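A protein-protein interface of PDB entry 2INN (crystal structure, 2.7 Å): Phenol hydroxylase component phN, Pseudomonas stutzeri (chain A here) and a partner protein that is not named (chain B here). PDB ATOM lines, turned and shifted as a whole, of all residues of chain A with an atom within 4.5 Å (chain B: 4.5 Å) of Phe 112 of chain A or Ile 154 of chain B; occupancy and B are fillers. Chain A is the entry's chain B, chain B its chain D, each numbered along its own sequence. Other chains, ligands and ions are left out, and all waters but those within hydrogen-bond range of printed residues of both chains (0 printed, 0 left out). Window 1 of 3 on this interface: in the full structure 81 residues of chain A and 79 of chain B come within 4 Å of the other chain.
Among the printed residues, pairs that only touch across the chains: Phe 112 of chain A with Ser 150 of chain B (3.6 Å), Phe 112 of chain A with Ile 154 of chain B (3.99 Å), Ile 136 of chain A with Met 158 of chain B (3.8 Å) and Leu 139 of chain A with Tyr 155 of chain B (3.4 Å).
Printed residues of chain A within 4 Å of Ile 154 of chain B: Phe 112. Of the printed residues of chain A, Met 158 of chain B touches Ile 136 (3.8 Å). Of the printed residues of chain B, Ile 136 of chain A touches Met 158 (3.8 Å). Printed residues of chain B within 4 Å of Leu 139 of chain A: Tyr 155 (3.4 Å). Of the printed residues of chain A, Ser 150 of chain B touches Phe 112 (3.6 Å). The nearest printed residue of chain B that does not touch Phe 112 of chain A is Gln 151 of chain B (4.1 Å). The nearest printed residue of chain A that does not touch Tyr 155 of chain B is Ile 136 of chain A (4.3 Å).
Of the 10 printed residues of chain B, 4 touch a printed residue of chain A. Printed residues of chain B that touch a printed residue of chain A: Ser 150, Ile 154, Tyr 155 and Met 158. Among the printed residues, no Asp or Glu carboxylate lies within 4 Å of a Lys or Arg side-chain nitrogen of the other chain.
The side-chain hydroxyl (OH) of Tyr 155 of chain B sits at hydrogen-bond distance from the side-chain amide nitrogen (NE2) of Gln 151 of chain B, 2.6 Å away. O of Phe 112 of chain A is in hydrogen-bond range of OG of Ser 116 of chain A.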
ATOM      1  N   GLU A 108     -13.043  13.456  29.152  1.00  0.00           N
ATOM      2  CA  GLU A 108     -13.585  14.052  27.917  1.00  0.00           C
ATOM      3  C   GLU A 108     -12.764  15.279  27.576  1.00  0.00           C
ATOM      4  O   GLU A 108     -12.413  15.559  26.444  1.00  0.00           O
ATOM      5  CB  GLU A 108     -15.085  14.392  28.037  1.00  0.00           C
ATOM      6  CG  GLU A 108     -15.987  13.239  28.444  1.00  0.00           C
ATOM      7  CD  GLU A 108     -16.271  12.239  27.302  1.00  0.00           C
ATOM      8  OE1 GLU A 108     -15.640  12.282  26.207  1.00  0.00           O
ATOM      9  OE2 GLU A 108     -17.153  11.380  27.527  1.00  0.00           O
ATOM     10  N   HIS A 109     -12.416  16.012  28.600  1.00  0.00           N
ATOM     11  CA  HIS A 109     -11.494  17.138  28.415  1.00  0.00           C
ATOM     12  C   HIS A 109     -10.065  16.746  27.939  1.00  0.00           C
ATOM     13  O   HIS A 109      -9.454  17.406  27.052  1.00  0.00           O
ATOM     14  CB  HIS A 109     -11.460  18.025  29.679  1.00  0.00           C
ATOM     15  CG  HIS A 109     -11.470  19.477  29.370  1.00  0.00           C
ATOM     16  ND1 HIS A 109     -12.607  20.129  28.993  1.00  0.00           N
ATOM     17  CD2 HIS A 109     -10.472  20.394  29.324  1.00  0.00           C
ATOM     18  CE1 HIS A 109     -12.315  21.410  28.762  1.00  0.00           C
ATOM     19  NE2 HIS A 109     -11.020  21.599  28.961  1.00  0.00           N
ATOM     20  N   ALA A 110      -9.523  15.681  28.526  1.00  0.00           N
ATOM     21  CA  ALA A 110      -8.199  15.322  28.155  1.00  0.00           C
ATOM     22  C   ALA A 110      -8.339  14.866  26.692  1.00  0.00           C
ATOM     23  O   ALA A 110      -7.477  15.194  25.916  1.00  0.00           O
ATOM     24  CB  ALA A 110      -7.655  14.288  29.068  1.00  0.00           C
ATOM     25  N   ALA A 111      -9.442  14.251  26.262  1.00  0.00           N
ATOM     26  CA  ALA A 111      -9.547  13.962  24.824  1.00  0.00           C
ATOM     27  C   ALA A 111      -9.486  15.205  23.921  1.00  0.00           C
ATOM     28  O   ALA A 111      -8.855  15.236  22.802  1.00  0.00           O
ATOM     29  CB  ALA A 111     -10.810  13.238  24.516  1.00  0.00           C
ATOM     30  N   PHE A 112     -10.173  16.227  24.413  1.00  0.00           N
ATOM     31  CA  PHE A 112     -10.325  17.436  23.648  1.00  0.00           C
ATOM     32  C   PHE A 112      -8.901  17.960  23.471  1.00  0.00           C
ATOM     33  O   PHE A 112      -8.462  18.129  22.345  1.00  0.00           O
ATOM     34  CB  PHE A 112     -11.291  18.403  24.366  1.00  0.00           C
ATOM     35  CG  PHE A 112     -10.986  19.816  24.124  1.00  0.00           C
ATOM     36  CD1 PHE A 112     -11.059  20.355  22.810  1.00  0.00           C
ATOM     37  CD2 PHE A 112     -10.528  20.627  25.181  1.00  0.00           C
ATOM     38  CE1 PHE A 112     -10.729  21.773  22.561  1.00  0.00           C
ATOM     39  CE2 PHE A 112     -10.135  22.065  24.972  1.00  0.00           C
ATOM     40  CZ  PHE A 112     -10.242  22.616  23.682  1.00  0.00           C
ATOM     41  N   GLN A 113      -8.157  18.133  24.562  1.00  0.00           N
ATOM     42  CA  GLN A 113      -6.743  18.449  24.450  1.00  0.00           C
ATOM     43  C   GLN A 113      -5.991  17.479  23.512  1.00  0.00           C
ATOM     44  O   GLN A 113      -5.502  17.874  22.466  1.00  0.00           O
ATOM     45  CB  GLN A 113      -6.106  18.522  25.842  1.00  0.00           C
ATOM     46  CG  GLN A 113      -6.170  19.977  26.479  1.00  0.00           C
ATOM     47  CD  GLN A 113      -5.940  20.018  28.025  1.00  0.00           C
ATOM     48  OE1 GLN A 113      -5.971  19.026  28.721  1.00  0.00           O
ATOM     49  NE2 GLN A 113      -5.718  21.201  28.533  1.00  0.00           N
ATOM     50  N   GLY A 114      -5.892  16.205  23.856  1.00  0.00           N
ATOM     51  CA  GLY A 114      -5.271  15.232  22.933  1.00  0.00           C
ATOM     52  C   GLY A 114      -5.528  15.404  21.441  1.00  0.00           C
ATOM     53  O   GLY A 114      -4.585  15.615  20.654  1.00  0.00           O
ATOM     54  N   TYR A 115      -6.811  15.386  21.062  1.00  0.00           N
ATOM     55  CA  TYR A 115      -7.170  15.462  19.641  1.00  0.00           C
ATOM     56  C   TYR A 115      -6.896  16.813  18.923  1.00  0.00           C
ATOM     57  O   TYR A 115      -6.450  16.842  17.776  1.00  0.00           O
ATOM     58  CB  TYR A 115      -8.612  15.039  19.474  1.00  0.00           C
ATOM     59  CG  TYR A 115      -8.833  13.563  19.552  1.00  0.00           C
ATOM     60  CD1 TYR A 115      -9.311  12.969  20.693  1.00  0.00           C
ATOM     61  CD2 TYR A 115      -8.539  12.748  18.472  1.00  0.00           C
ATOM     62  CE1 TYR A 115      -9.514  11.670  20.747  1.00  0.00           C
ATOM     63  CE2 TYR A 115      -8.749  11.389  18.507  1.00  0.00           C
ATOM     64  CZ  TYR A 115      -9.239  10.851  19.636  1.00  0.00           C
ATOM     65  OH  TYR A 115      -9.434   9.446  19.666  1.00  0.00           O
ATOM     66  N   SER A 116      -7.181  17.929  19.595  1.00  0.00           N
ATOM     67  CA  SER A 116      -6.710  19.240  19.138  1.00  0.00           C
ATOM     68  C   SER A 116      -5.240  19.097  18.719  1.00  0.00           C
ATOM     69  O   SER A 116      -4.903  19.407  17.550  1.00  0.00           O
ATOM     70  CB  SER A 116      -6.794  20.328  20.250  1.00  0.00           C
ATOM     71  OG  SER A 116      -8.063  20.357  20.930  1.00  0.00           O
ATOM     72  N   ALA A 135     -11.910  16.182  18.295  1.00  0.00           N
ATOM     73  CA  ALA A 135     -11.484  17.070  19.293  1.00  0.00           C
ATOM     74  C   ALA A 135     -12.634  18.012  19.755  1.00  0.00           C
ATOM     75  O   ALA A 135     -12.711  18.410  20.927  1.00  0.00           O
ATOM     76  CB  ALA A 135     -10.387  17.857  18.734  1.00  0.00           C
ATOM     77  N   ILE A 136     -13.500  18.427  18.851  1.00  0.00           N
ATOM     78  CA  ILE A 136     -14.468  19.408  19.232  1.00  0.00           C
ATOM     79  C   ILE A 136     -15.658  18.688  19.840  1.00  0.00           C
ATOM     80  O   ILE A 136     -16.229  19.211  20.794  1.00  0.00           O
ATOM     81  CB  ILE A 136     -14.853  20.388  18.039  1.00  0.00           C
ATOM     82  CG1 ILE A 136     -15.687  21.600  18.498  1.00  0.00           C
ATOM     83  CG2 ILE A 136     -15.480  19.677  16.773  1.00  0.00           C
ATOM     84  CD1 ILE A 136     -16.190  22.312  17.339  1.00  0.00           C
ATOM     85  N   GLU A 138     -15.204  16.200  21.747  1.00  0.00           N
ATOM     86  CA  GLU A 138     -14.874  15.880  23.117  1.00  0.00           C
ATOM     87  C   GLU A 138     -15.186  17.083  24.033  1.00  0.00           C
ATOM     88  O   GLU A 138     -15.648  16.966  25.222  1.00  0.00           O
ATOM     89  CB  GLU A 138     -13.468  15.274  23.248  1.00  0.00           C
ATOM     90  CG  GLU A 138     -13.292  13.930  22.392  1.00  0.00           C
ATOM     91  CD  GLU A 138     -13.993  12.815  22.998  1.00  0.00           C
ATOM     92  OE1 GLU A 138     -13.905  11.643  22.545  1.00  0.00           O
ATOM     93  OE2 GLU A 138     -14.649  13.087  24.015  1.00  0.00           O
ATOM     94  N   LEU A 139     -14.995  18.264  23.463  1.00  0.00           N
ATOM     95  CA  LEU A 139     -15.148  19.418  24.291  1.00  0.00           C
ATOM     96  C   LEU A 139     -16.653  19.499  24.611  1.00  0.00           C
ATOM     97  O   LEU A 139     -17.011  19.750  25.773  1.00  0.00           O
ATOM     98  CB  LEU A 139     -14.661  20.625  23.547  1.00  0.00           C
ATOM     99  CG  LEU A 139     -15.110  21.956  24.132  1.00  0.00           C
ATOM    100  CD1 LEU A 139     -14.413  22.175  25.496  1.00  0.00           C
ATOM    101  CD2 LEU A 139     -14.909  23.107  23.147  1.00  0.00           C
ATOM    102  N   ALA B 141      -5.093  25.437  20.090  1.00  0.00           N
ATOM    103  CA  ALA B 141      -6.155  24.897  20.925  1.00  0.00           C
ATOM    104  C   ALA B 141      -5.492  23.855  21.740  1.00  0.00           C
ATOM    105  O   ALA B 141      -5.904  23.647  22.856  1.00  0.00           O
ATOM    106  CB  ALA B 141      -7.281  24.327  20.151  1.00  0.00           C
ATOM    107  N   SER B 150      -8.600  28.121  25.091  1.00  0.00           N
ATOM    108  CA  SER B 150      -8.336  27.069  24.146  1.00  0.00           C
ATOM    109  C   SER B 150      -9.549  26.852  23.240  1.00  0.00           C
ATOM    110  O   SER B 150      -9.373  26.804  22.024  1.00  0.00           O
ATOM    111  CB  SER B 150      -7.933  25.767  24.833  1.00  0.00           C
ATOM    112  OG  SER B 150      -9.015  25.425  25.649  1.00  0.00           O
ATOM    113  N   GLN B 151     -10.716  26.702  23.862  1.00  0.00           N
ATOM    114  CA  GLN B 151     -12.018  26.663  23.279  1.00  0.00           C
ATOM    115  C   GLN B 151     -12.128  27.700  22.157  1.00  0.00           C
ATOM    116  O   GLN B 151     -12.478  27.356  21.032  1.00  0.00           O
ATOM    117  CB  GLN B 151     -12.990  26.930  24.409  1.00  0.00           C
ATOM    118  CG  GLN B 151     -14.289  27.505  24.020  1.00  0.00           C
ATOM    119  CD  GLN B 151     -15.382  27.394  25.176  1.00  0.00           C
ATOM    120  OE1 GLN B 151     -15.295  28.088  26.243  1.00  0.00           O
ATOM    121  NE2 GLN B 151     -16.418  26.550  24.938  1.00  0.00           N
ATOM    122  N   MET B 152     -11.730  28.955  22.413  1.00  0.00           N
ATOM    123  CA  MET B 152     -11.876  29.927  21.406  1.00  0.00           C
ATOM    124  C   MET B 152     -11.107  29.637  20.152  1.00  0.00           C
ATOM    125  O   MET B 152     -11.505  29.993  19.049  1.00  0.00           O
ATOM    126  CB  MET B 152     -11.506  31.243  21.967  1.00  0.00           C
ATOM    127  CG  MET B 152     -12.739  32.073  22.314  1.00  0.00           C
ATOM    128  SD  MET B 152     -12.157  33.562  23.450  1.00  0.00           S
ATOM    129  CE  MET B 152     -13.603  34.482  23.510  1.00  0.00           C
ATOM    130  N   HIS B 153      -9.985  28.967  20.295  1.00  0.00           N
ATOM    131  CA  HIS B 153      -9.111  28.642  19.158  1.00  0.00           C
ATOM    132  C   HIS B 153      -9.610  27.465  18.345  1.00  0.00           C
ATOM    133  O   HIS B 153      -9.470  27.427  17.120  1.00  0.00           O
ATOM    134  CB  HIS B 153      -7.706  28.478  19.679  1.00  0.00           C
ATOM    135  CG  HIS B 153      -7.107  29.786  20.055  1.00  0.00           C
ATOM    136  ND1 HIS B 153      -7.361  30.384  21.267  1.00  0.00           N
ATOM    137  CD2 HIS B 153      -6.373  30.681  19.331  1.00  0.00           C
ATOM    138  CE1 HIS B 153      -6.769  31.574  21.286  1.00  0.00           C
ATOM    139  NE2 HIS B 153      -6.156  31.782  20.128  1.00  0.00           N
ATOM    140  N   ILE B 154     -10.275  26.545  19.024  1.00  0.00           N
ATOM    141  CA  ILE B 154     -10.877  25.415  18.331  1.00  0.00           C
ATOM    142  C   ILE B 154     -12.124  25.824  17.471  1.00  0.00           C
ATOM    143  O   ILE B 154     -12.193  25.449  16.281  1.00  0.00           O
ATOM    144  CB  ILE B 154     -11.105  24.209  19.277  1.00  0.00           C
ATOM    145  CG1 ILE B 154     -11.074  22.889  18.484  1.00  0.00           C
ATOM    146  CG2 ILE B 154     -12.453  24.228  19.933  1.00  0.00           C
ATOM    147  CD1 ILE B 154      -9.868  22.681  17.586  1.00  0.00           C
ATOM    148  N   TYR B 155     -13.019  26.644  18.051  1.00  0.00           N
ATOM    149  CA  TYR B 155     -14.092  27.259  17.353  1.00  0.00           C
ATOM    150  C   TYR B 155     -13.579  27.996  16.156  1.00  0.00           C
ATOM    151  O   TYR B 155     -13.993  27.776  15.034  1.00  0.00           O
ATOM    152  CB  TYR B 155     -14.821  28.192  18.271  1.00  0.00           C
ATOM    153  CG  TYR B 155     -15.491  27.425  19.411  1.00  0.00           C
ATOM    154  CD1 TYR B 155     -15.724  28.037  20.616  1.00  0.00           C
ATOM    155  CD2 TYR B 155     -15.808  26.088  19.304  1.00  0.00           C
ATOM    156  CE1 TYR B 155     -16.256  27.388  21.695  1.00  0.00           C
ATOM    157  CE2 TYR B 155     -16.362  25.408  20.388  1.00  0.00           C
ATOM    158  CZ  TYR B 155     -16.589  26.095  21.573  1.00  0.00           C
ATOM    159  OH  TYR B 155     -17.178  25.541  22.662  1.00  0.00           O
ATOM    160  N   THR B 156     -12.560  28.777  16.320  1.00  0.00           N
ATOM    161  CA  THR B 156     -12.238  29.576  15.189  1.00  0.00           C
ATOM    162  C   THR B 156     -11.534  28.793  14.108  1.00  0.00           C
ATOM    163  O   THR B 156     -11.544  29.196  12.931  1.00  0.00           O
ATOM    164  CB  THR B 156     -11.516  30.790  15.640  1.00  0.00           C
ATOM    165  OG1 THR B 156     -11.693  31.811  14.659  1.00  0.00           O
ATOM    166  CG2 THR B 156     -10.109  30.523  15.884  1.00  0.00           C
ATOM    167  N   GLY B 157     -10.896  27.666  14.500  1.00  0.00           N
ATOM    168  CA  GLY B 157     -10.043  26.929  13.607  1.00  0.00           C
ATOM    169  C   GLY B 157     -11.063  26.224  12.769  1.00  0.00           C
ATOM    170  O   GLY B 157     -10.940  26.160  11.532  1.00  0.00           O
ATOM    171  N   MET B 158     -12.076  25.695  13.454  1.00  0.00           N
ATOM    172  CA  MET B 158     -13.211  25.041  12.758  1.00  0.00           C
ATOM    173  C   MET B 158     -13.835  25.954  11.751  1.00  0.00           C
ATOM    174  O   MET B 158     -14.104  25.481  10.663  1.00  0.00           O
ATOM    175  CB  MET B 158     -14.306  24.531  13.710  1.00  0.00           C
ATOM    176  CG  MET B 158     -13.809  23.376  14.635  1.00  0.00           C
ATOM    177  SD  MET B 158     -13.037  21.839  13.564  1.00  0.00           S
ATOM    178  CE  MET B 158     -11.148  22.354  13.461  1.00  0.00           C
